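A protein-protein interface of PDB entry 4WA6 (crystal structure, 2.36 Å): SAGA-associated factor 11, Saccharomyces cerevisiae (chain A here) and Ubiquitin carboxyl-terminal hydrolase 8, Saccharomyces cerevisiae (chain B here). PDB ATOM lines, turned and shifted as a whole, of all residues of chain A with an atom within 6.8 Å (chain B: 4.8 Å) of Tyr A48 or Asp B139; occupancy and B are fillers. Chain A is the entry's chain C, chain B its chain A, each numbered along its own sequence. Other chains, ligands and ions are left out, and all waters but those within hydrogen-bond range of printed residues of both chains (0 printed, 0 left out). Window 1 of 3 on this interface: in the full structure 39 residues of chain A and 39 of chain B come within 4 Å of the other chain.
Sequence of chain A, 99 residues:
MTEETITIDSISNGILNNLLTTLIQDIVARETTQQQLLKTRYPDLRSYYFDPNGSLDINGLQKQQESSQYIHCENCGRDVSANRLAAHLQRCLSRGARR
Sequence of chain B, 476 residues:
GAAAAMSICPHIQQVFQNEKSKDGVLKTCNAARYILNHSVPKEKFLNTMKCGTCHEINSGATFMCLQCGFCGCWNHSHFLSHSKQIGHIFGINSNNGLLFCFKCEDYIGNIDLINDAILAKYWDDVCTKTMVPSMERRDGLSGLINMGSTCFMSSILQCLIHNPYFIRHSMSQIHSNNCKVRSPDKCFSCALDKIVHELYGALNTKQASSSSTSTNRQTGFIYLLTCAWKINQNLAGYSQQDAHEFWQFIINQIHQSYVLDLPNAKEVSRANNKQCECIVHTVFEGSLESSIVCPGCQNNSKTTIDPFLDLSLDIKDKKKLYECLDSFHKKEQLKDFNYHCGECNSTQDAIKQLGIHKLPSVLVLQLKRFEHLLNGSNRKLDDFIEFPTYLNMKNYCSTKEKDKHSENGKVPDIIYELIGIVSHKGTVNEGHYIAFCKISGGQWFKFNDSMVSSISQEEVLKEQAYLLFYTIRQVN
Printed residues of chain B that touch a printed residue of chain A: Met B135, Arg B138, Asp B139, Leu B141 and Phe B445. Hydrophobic or aromatic side chains of chain B within 4 Å of the printed part of chain A: Met B135, Leu B141 and Phe B445. Hydrophobic or aromatic side chains of chain A within 4 Å of the printed part of chain B: Leu A38, Tyr A48 and Ile A58. Among the printed residues, no Asp or Glu carboxylate lies within 4 Å of a Lys or Arg side-chain nitrogen of the other chain.
SD of Met B135 lies within hydrogen-bond range of N of Arg A46 (3.8 Å). NH1 of Arg B138 lies within hydrogen-bond range of OH of Tyr A48 (3.4 Å). OD2 of Asp B139 sits close to OH of Tyr A48 (2.3 Å).
Of the printed residues of chain B, Tyr A48 touches Arg B138, Asp B139, Leu B141 and Phe B445. Of chain A, only Tyr A48 (2.3 Å) comes within 4 Å of Asp B139. Of the printed residues of chain A, Met B135 touches Arg A46. Printed residues of chain A within 4 Å of Phe B445: Tyr A48 (3.8 Å) and Ile A58 (3.9 Å). Printed residues of chain A within 4 Å of Arg B138: Leu A38 and Tyr A48. Printed residues of chain B within 4 Å of Leu A38: Arg B138. Asn A59 touches none of the printed residues of chain B.
The guanidinium group of Arg B138 is in hydrogen-bond range of the backbone carbonyl oxygen of Met B135 (2.5 Å). The backbone carbonyl oxygen of Leu B141 sits at hydrogen-bond distance from the guanidinium group of Arg B137 (3.1 Å). The guanidinium group (NE) of Arg B138 lies within salt-bridge range of the side-chain carboxylate (OD2) of Asp B139 (3.9 Å). O of Asp B139 lies within hydrogen-bond range of NE2 of His B162 (3.3 Å). The backbone NH of Tyr A49 is in hydrogen-bond range of the backbone carbonyl oxygen of Ile A58, 2.9 Å away.
Arg B138 touches Leu A38 (NE to CD2, 3.7 Å). CE1 of Tyr A48 touches CD1 of Leu B141, at 3.8 Å. Phe B445 touches Tyr A48 (CZ to CD2, 3.8 Å). Ile A58 touches Phe B445 (CG2 to CE1, 3.9 Å).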
ATOM      1  N   LEU A  38      -2.258 -16.878 -21.199  1.00  0.00           N
ATOM      2  CA  LEU A  38      -1.109 -17.622 -20.782  1.00  0.00           C
ATOM      3  C   LEU A  38      -1.496 -19.038 -20.331  1.00  0.00           C
ATOM      4  O   LEU A  38      -0.796 -19.991 -20.643  1.00  0.00           O
ATOM      5  CB  LEU A  38      -0.375 -16.908 -19.656  1.00  0.00           C
ATOM      6  CG  LEU A  38       0.445 -15.694 -20.009  1.00  0.00           C
ATOM      7  CD1 LEU A  38       1.105 -15.177 -18.718  1.00  0.00           C
ATOM      8  CD2 LEU A  38       1.492 -15.976 -21.075  1.00  0.00           C
ATOM      9  N   ARG A  46       4.358 -23.226 -15.524  1.00  0.00           N
ATOM     10  CA  ARG A  46       4.910 -22.842 -14.217  1.00  0.00           C
ATOM     11  C   ARG A  46       5.097 -21.316 -14.161  1.00  0.00           C
ATOM     12  O   ARG A  46       5.476 -20.716 -15.153  1.00  0.00           O
ATOM     13  CB  ARG A  46       6.256 -23.510 -13.984  1.00  0.00           C
ATOM     14  CG  ARG A  46       6.151 -24.981 -13.623  1.00  0.00           C
ATOM     15  CD  ARG A  46       7.479 -25.701 -13.791  1.00  0.00           C
ATOM     16  NE  ARG A  46       8.165 -25.355 -15.040  1.00  0.00           N
ATOM     17  CZ  ARG A  46       7.813 -25.780 -16.256  1.00  0.00           C
ATOM     18  NH1 ARG A  46       6.749 -26.566 -16.434  1.00  0.00           N
ATOM     19  NH2 ARG A  46       8.521 -25.400 -17.314  1.00  0.00           N
ATOM     20  N   SER A  47       4.820 -20.700 -13.012  1.00  0.00           N
ATOM     21  CA  SER A  47       5.245 -19.328 -12.768  1.00  0.00           C
ATOM     22  C   SER A  47       6.740 -19.312 -12.493  1.00  0.00           C
ATOM     23  O   SER A  47       7.365 -20.357 -12.426  1.00  0.00           O
ATOM     24  CB  SER A  47       4.449 -18.649 -11.640  1.00  0.00           C
ATOM     25  OG  SER A  47       4.100 -19.569 -10.643  1.00  0.00           O
ATOM     26  N   TYR A  48       7.315 -18.118 -12.409  1.00  0.00           N
ATOM     27  CA  TYR A  48       8.746 -18.007 -12.208  1.00  0.00           C
ATOM     28  C   TYR A  48       9.019 -18.197 -10.720  1.00  0.00           C
ATOM     29  O   TYR A  48       8.268 -17.681  -9.860  1.00  0.00           O
ATOM     30  CB  TYR A  48       9.263 -16.663 -12.727  1.00  0.00           C
ATOM     31  CG  TYR A  48       9.112 -16.448 -14.249  1.00  0.00           C
ATOM     32  CD1 TYR A  48       9.926 -17.118 -15.158  1.00  0.00           C
ATOM     33  CD2 TYR A  48       8.172 -15.553 -14.763  1.00  0.00           C
ATOM     34  CE1 TYR A  48       9.808 -16.897 -16.523  1.00  0.00           C
ATOM     35  CE2 TYR A  48       8.030 -15.351 -16.131  1.00  0.00           C
ATOM     36  CZ  TYR A  48       8.859 -16.027 -17.007  1.00  0.00           C
ATOM     37  OH  TYR A  48       8.731 -15.834 -18.369  1.00  0.00           O
ATOM     38  N   TYR A  49      10.063 -18.973 -10.418  1.00  0.00           N
ATOM     39  CA  TYR A  49      10.413 -19.293  -9.035  1.00  0.00           C
ATOM     40  C   TYR A  49      10.950 -18.103  -8.213  1.00  0.00           C
ATOM     41  O   TYR A  49      11.741 -17.307  -8.723  1.00  0.00           O
ATOM     42  CB  TYR A  49      11.463 -20.386  -9.010  1.00  0.00           C
ATOM     43  CG  TYR A  49      11.613 -20.941  -7.628  1.00  0.00           C
ATOM     44  CD1 TYR A  49      12.520 -20.381  -6.721  1.00  0.00           C
ATOM     45  CD2 TYR A  49      10.815 -21.985  -7.203  1.00  0.00           C
ATOM     46  CE1 TYR A  49      12.633 -20.872  -5.436  1.00  0.00           C
ATOM     47  CE2 TYR A  49      10.925 -22.485  -5.924  1.00  0.00           C
ATOM     48  CZ  TYR A  49      11.829 -21.926  -5.042  1.00  0.00           C
ATOM     49  OH  TYR A  49      11.934 -22.435  -3.769  1.00  0.00           O
ATOM     50  N   PHE A  50      10.547 -18.014  -6.940  1.00  0.00           N
ATOM     51  CA  PHE A  50      10.984 -16.934  -6.055  1.00  0.00           C
ATOM     52  C   PHE A  50      11.600 -17.451  -4.769  1.00  0.00           C
ATOM     53  O   PHE A  50      10.893 -17.884  -3.878  1.00  0.00           O
ATOM     54  CB  PHE A  50       9.850 -15.956  -5.690  1.00  0.00           C
ATOM     55  CG  PHE A  50      10.263 -14.968  -4.624  1.00  0.00           C
ATOM     56  CD1 PHE A  50      11.009 -13.841  -4.958  1.00  0.00           C
ATOM     57  CD2 PHE A  50       9.993 -15.217  -3.265  1.00  0.00           C
ATOM     58  CE1 PHE A  50      11.429 -12.962  -3.977  1.00  0.00           C
ATOM     59  CE2 PHE A  50      10.407 -14.338  -2.278  1.00  0.00           C
ATOM     60  CZ  PHE A  50      11.128 -13.207  -2.634  1.00  0.00           C
ATOM     61  N   ASP A  57      17.659 -19.247  -8.803  1.00  0.00           N
ATOM     62  CA  ASP A  57      17.180 -18.555 -10.029  1.00  0.00           C
ATOM     63  C   ASP A  57      15.715 -18.885 -10.358  1.00  0.00           C
ATOM     64  O   ASP A  57      14.991 -19.465  -9.532  1.00  0.00           O
ATOM     65  CB  ASP A  57      18.102 -18.860 -11.238  1.00  0.00           C
ATOM     66  CG  ASP A  57      17.845 -20.216 -11.845  1.00  0.00           C
ATOM     67  OD1 ASP A  57      16.832 -20.845 -11.452  1.00  0.00           O
ATOM     68  OD2 ASP A  57      18.678 -20.664 -12.685  1.00  0.00           O
ATOM     69  N   ILE A  58      15.281 -18.541 -11.569  1.00  0.00           N
ATOM     70  CA  ILE A  58      13.846 -18.550 -11.875  1.00  0.00           C
ATOM     71  C   ILE A  58      13.293 -19.958 -12.113  1.00  0.00           C
ATOM     72  O   ILE A  58      12.062 -20.131 -12.144  1.00  0.00           O
ATOM     73  CB  ILE A  58      13.481 -17.619 -13.051  1.00  0.00           C
ATOM     74  CG1 ILE A  58      14.322 -17.933 -14.292  1.00  0.00           C
ATOM     75  CG2 ILE A  58      13.637 -16.156 -12.623  1.00  0.00           C
ATOM     76  CD1 ILE A  58      14.072 -17.016 -15.460  1.00  0.00           C
ATOM     77  N   ASN A  59      14.187 -20.935 -12.286  1.00  0.00           N
ATOM     78  CA  ASN A  59      13.810 -22.374 -12.272  1.00  0.00           C
ATOM     79  C   ASN A  59      14.175 -23.088 -10.970  1.00  0.00           C
ATOM     80  O   ASN A  59      14.415 -24.294 -10.945  1.00  0.00           O
ATOM     81  CB  ASN A  59      14.403 -23.065 -13.505  1.00  0.00           C
ATOM     82  CG  ASN A  59      14.164 -22.240 -14.740  1.00  0.00           C
ATOM     83  OD1 ASN A  59      13.018 -21.846 -15.001  1.00  0.00           O
ATOM     84  ND2 ASN A  59      15.244 -21.830 -15.417  1.00  0.00           N
ATOM     85  N   GLY A  60      14.208 -22.324  -9.881  1.00  0.00           N
ATOM     86  CA  GLY A  60      14.626 -22.830  -8.575  1.00  0.00           C
ATOM     87  C   GLY A  60      16.018 -23.448  -8.516  1.00  0.00           C
ATOM     88  O   GLY A  60      16.265 -24.304  -7.675  1.00  0.00           O
ATOM     89  N   MET B 135       7.073 -21.337 -23.813  1.00  0.00           N
ATOM     90  CA  MET B 135       6.914 -20.906 -22.429  1.00  0.00           C
ATOM     91  C   MET B 135       8.183 -20.303 -21.810  1.00  0.00           C
ATOM     92  O   MET B 135       8.084 -19.377 -21.035  1.00  0.00           O
ATOM     93  CB  MET B 135       6.432 -22.108 -21.571  1.00  0.00           C
ATOM     94  CG  MET B 135       6.178 -21.795 -20.105  1.00  0.00           C
ATOM     95  SD  MET B 135       5.500 -23.139 -19.106  1.00  0.00           S
ATOM     96  CE  MET B 135       6.497 -24.532 -19.614  1.00  0.00           C
ATOM     97  N   ARG B 137      10.866 -18.923 -23.423  1.00  0.00           N
ATOM     98  CA  ARG B 137      11.457 -17.767 -24.136  1.00  0.00           C
ATOM     99  C   ARG B 137      10.537 -16.573 -24.202  1.00  0.00           C
ATOM    100  O   ARG B 137      10.933 -15.509 -24.700  1.00  0.00           O
ATOM    101  CB  ARG B 137      11.854 -18.144 -25.575  1.00  0.00           C
ATOM    102  CG  ARG B 137      12.744 -19.382 -25.722  1.00  0.00           C
ATOM    103  CD  ARG B 137      14.212 -19.172 -25.375  1.00  0.00           C
ATOM    104  NE  ARG B 137      14.547 -19.450 -23.973  1.00  0.00           N
ATOM    105  CZ  ARG B 137      14.915 -18.546 -23.056  1.00  0.00           C
ATOM    106  NH1 ARG B 137      15.016 -17.241 -23.314  1.00  0.00           N
ATOM    107  NH2 ARG B 137      15.199 -18.953 -21.840  1.00  0.00           N
ATOM    108  N   ARG B 138       9.328 -16.698 -23.676  1.00  0.00           N
ATOM    109  CA  ARG B 138       8.302 -15.733 -24.040  1.00  0.00           C
ATOM    110  C   ARG B 138       8.636 -14.345 -23.521  1.00  0.00           C
ATOM    111  O   ARG B 138       8.173 -13.371 -24.070  1.00  0.00           O
ATOM    112  CB  ARG B 138       6.898 -16.170 -23.586  1.00  0.00           C
ATOM    113  CG  ARG B 138       6.671 -16.066 -22.095  1.00  0.00           C
ATOM    114  CD  ARG B 138       5.390 -16.767 -21.672  1.00  0.00           C
ATOM    115  NE  ARG B 138       5.101 -16.544 -20.254  1.00  0.00           N
ATOM    116  CZ  ARG B 138       5.668 -17.195 -19.243  1.00  0.00           C
ATOM    117  NH1 ARG B 138       6.535 -18.137 -19.439  1.00  0.00           N
ATOM    118  NH2 ARG B 138       5.332 -16.934 -18.015  1.00  0.00           N
ATOM    119  N   ASP B 139       9.430 -14.234 -22.464  1.00  0.00           N
ATOM    120  CA  ASP B 139       9.790 -12.890 -21.944  1.00  0.00           C
ATOM    121  C   ASP B 139      11.278 -12.638 -22.172  1.00  0.00           C
ATOM    122  O   ASP B 139      11.828 -11.677 -21.639  1.00  0.00           O
ATOM    123  CB  ASP B 139       9.474 -12.774 -20.456  1.00  0.00           C
ATOM    124  CG  ASP B 139       8.004 -13.081 -20.132  1.00  0.00           C
ATOM    125  OD1 ASP B 139       7.096 -12.563 -20.850  1.00  0.00           O
ATOM    126  OD2 ASP B 139       7.766 -13.855 -19.152  1.00  0.00           O
ATOM    127  N   GLY B 140      11.919 -13.495 -22.975  1.00  0.00           N
ATOM    128  CA  GLY B 140      13.315 -13.338 -23.299  1.00  0.00           C
ATOM    129  C   GLY B 140      14.236 -13.415 -22.107  1.00  0.00           C
ATOM    130  O   GLY B 140      15.348 -12.911 -22.168  1.00  0.00           O
ATOM    131  N   LEU B 141      13.809 -14.051 -21.022  1.00  0.00           N
ATOM    132  CA  LEU B 141      14.643 -14.100 -19.821  1.00  0.00           C
ATOM    133  C   LEU B 141      15.639 -15.168 -19.969  1.00  0.00           C
ATOM    134  O   LEU B 141      15.300 -16.237 -20.368  1.00  0.00           O
ATOM    135  CB  LEU B 141      13.852 -14.355 -18.550  1.00  0.00           C
ATOM    136  CG  LEU B 141      12.851 -13.285 -18.185  1.00  0.00           C
ATOM    137  CD1 LEU B 141      11.948 -13.800 -17.068  1.00  0.00           C
ATOM    138  CD2 LEU B 141      13.562 -11.998 -17.775  1.00  0.00           C
ATOM    139  N   HIS B 162      15.355  -5.872 -22.918  1.00  0.00           N
ATOM    140  CA  HIS B 162      14.066  -5.724 -22.250  1.00  0.00           C
ATOM    141  C   HIS B 162      13.514  -4.321 -22.412  1.00  0.00           C
ATOM    142  O   HIS B 162      12.473  -4.023 -21.908  1.00  0.00           O
ATOM    143  CB  HIS B 162      14.147  -6.162 -20.779  1.00  0.00           C
ATOM    144  CG  HIS B 162      14.404  -7.627 -20.631  1.00  0.00           C
ATOM    145  ND1 HIS B 162      15.613  -8.134 -20.199  1.00  0.00           N
ATOM    146  CD2 HIS B 162      13.636  -8.698 -20.924  1.00  0.00           C
ATOM    147  CE1 HIS B 162      15.573  -9.451 -20.210  1.00  0.00           C
ATOM    148  NE2 HIS B 162      14.386  -9.822 -20.656  1.00  0.00           N
ATOM    149  N   TYR B 200      14.454 -14.791 -27.377  1.00  0.00           N
ATOM    150  CA  TYR B 200      13.027 -14.758 -27.590  1.00  0.00           C
ATOM    151  C   TYR B 200      12.493 -15.821 -28.547  1.00  0.00           C
ATOM    152  O   TYR B 200      11.295 -16.132 -28.467  1.00  0.00           O
ATOM    153  CB  TYR B 200      12.595 -13.391 -28.077  1.00  0.00           C
ATOM    154  CG  TYR B 200      12.602 -12.329 -27.013  1.00  0.00           C
ATOM    155  CD1 TYR B 200      13.746 -11.552 -26.799  1.00  0.00           C
ATOM    156  CD2 TYR B 200      11.457 -12.064 -26.239  1.00  0.00           C
ATOM    157  CE1 TYR B 200      13.776 -10.561 -25.861  1.00  0.00           C
ATOM    158  CE2 TYR B 200      11.467 -11.068 -25.280  1.00  0.00           C
ATOM    159  CZ  TYR B 200      12.631 -10.306 -25.111  1.00  0.00           C
ATOM    160  OH  TYR B 200      12.687  -9.332 -24.174  1.00  0.00           O
ATOM    161  N   ILE B 439       9.355  -6.355 -16.787  1.00  0.00           N
ATOM    162  CA  ILE B 439       8.791  -6.840 -18.050  1.00  0.00           C
ATOM    163  C   ILE B 439       7.293  -6.649 -18.022  1.00  0.00           C
ATOM    164  O   ILE B 439       6.744  -6.137 -17.032  1.00  0.00           O
ATOM    165  CB  ILE B 439       9.147  -8.308 -18.275  1.00  0.00           C
ATOM    166  CG1 ILE B 439       8.210  -9.205 -17.479  1.00  0.00           C
ATOM    167  CG2 ILE B 439      10.582  -8.546 -17.845  1.00  0.00           C
ATOM    168  CD1 ILE B 439       8.522 -10.670 -17.607  1.00  0.00           C
ATOM    169  N   PHE B 445      13.067  -8.647 -12.533  1.00  0.00           N
ATOM    170  CA  PHE B 445      14.122  -9.640 -12.489  1.00  0.00           C
ATOM    171  C   PHE B 445      15.516  -9.078 -12.339  1.00  0.00           C
ATOM    172  O   PHE B 445      15.897  -8.105 -12.976  1.00  0.00           O
ATOM    173  CB  PHE B 445      14.090 -10.492 -13.753  1.00  0.00           C
ATOM    174  CG  PHE B 445      12.811 -11.179 -13.922  1.00  0.00           C
ATOM    175  CD1 PHE B 445      12.602 -12.425 -13.318  1.00  0.00           C
ATOM    176  CD2 PHE B 445      11.786 -10.564 -14.586  1.00  0.00           C
ATOM    177  CE1 PHE B 445      11.385 -13.075 -13.415  1.00  0.00           C
ATOM    178  CE2 PHE B 445      10.570 -11.203 -14.708  1.00  0.00           C
ATOM    179  CZ  PHE B 445      10.364 -12.470 -14.117  1.00  0.00           C
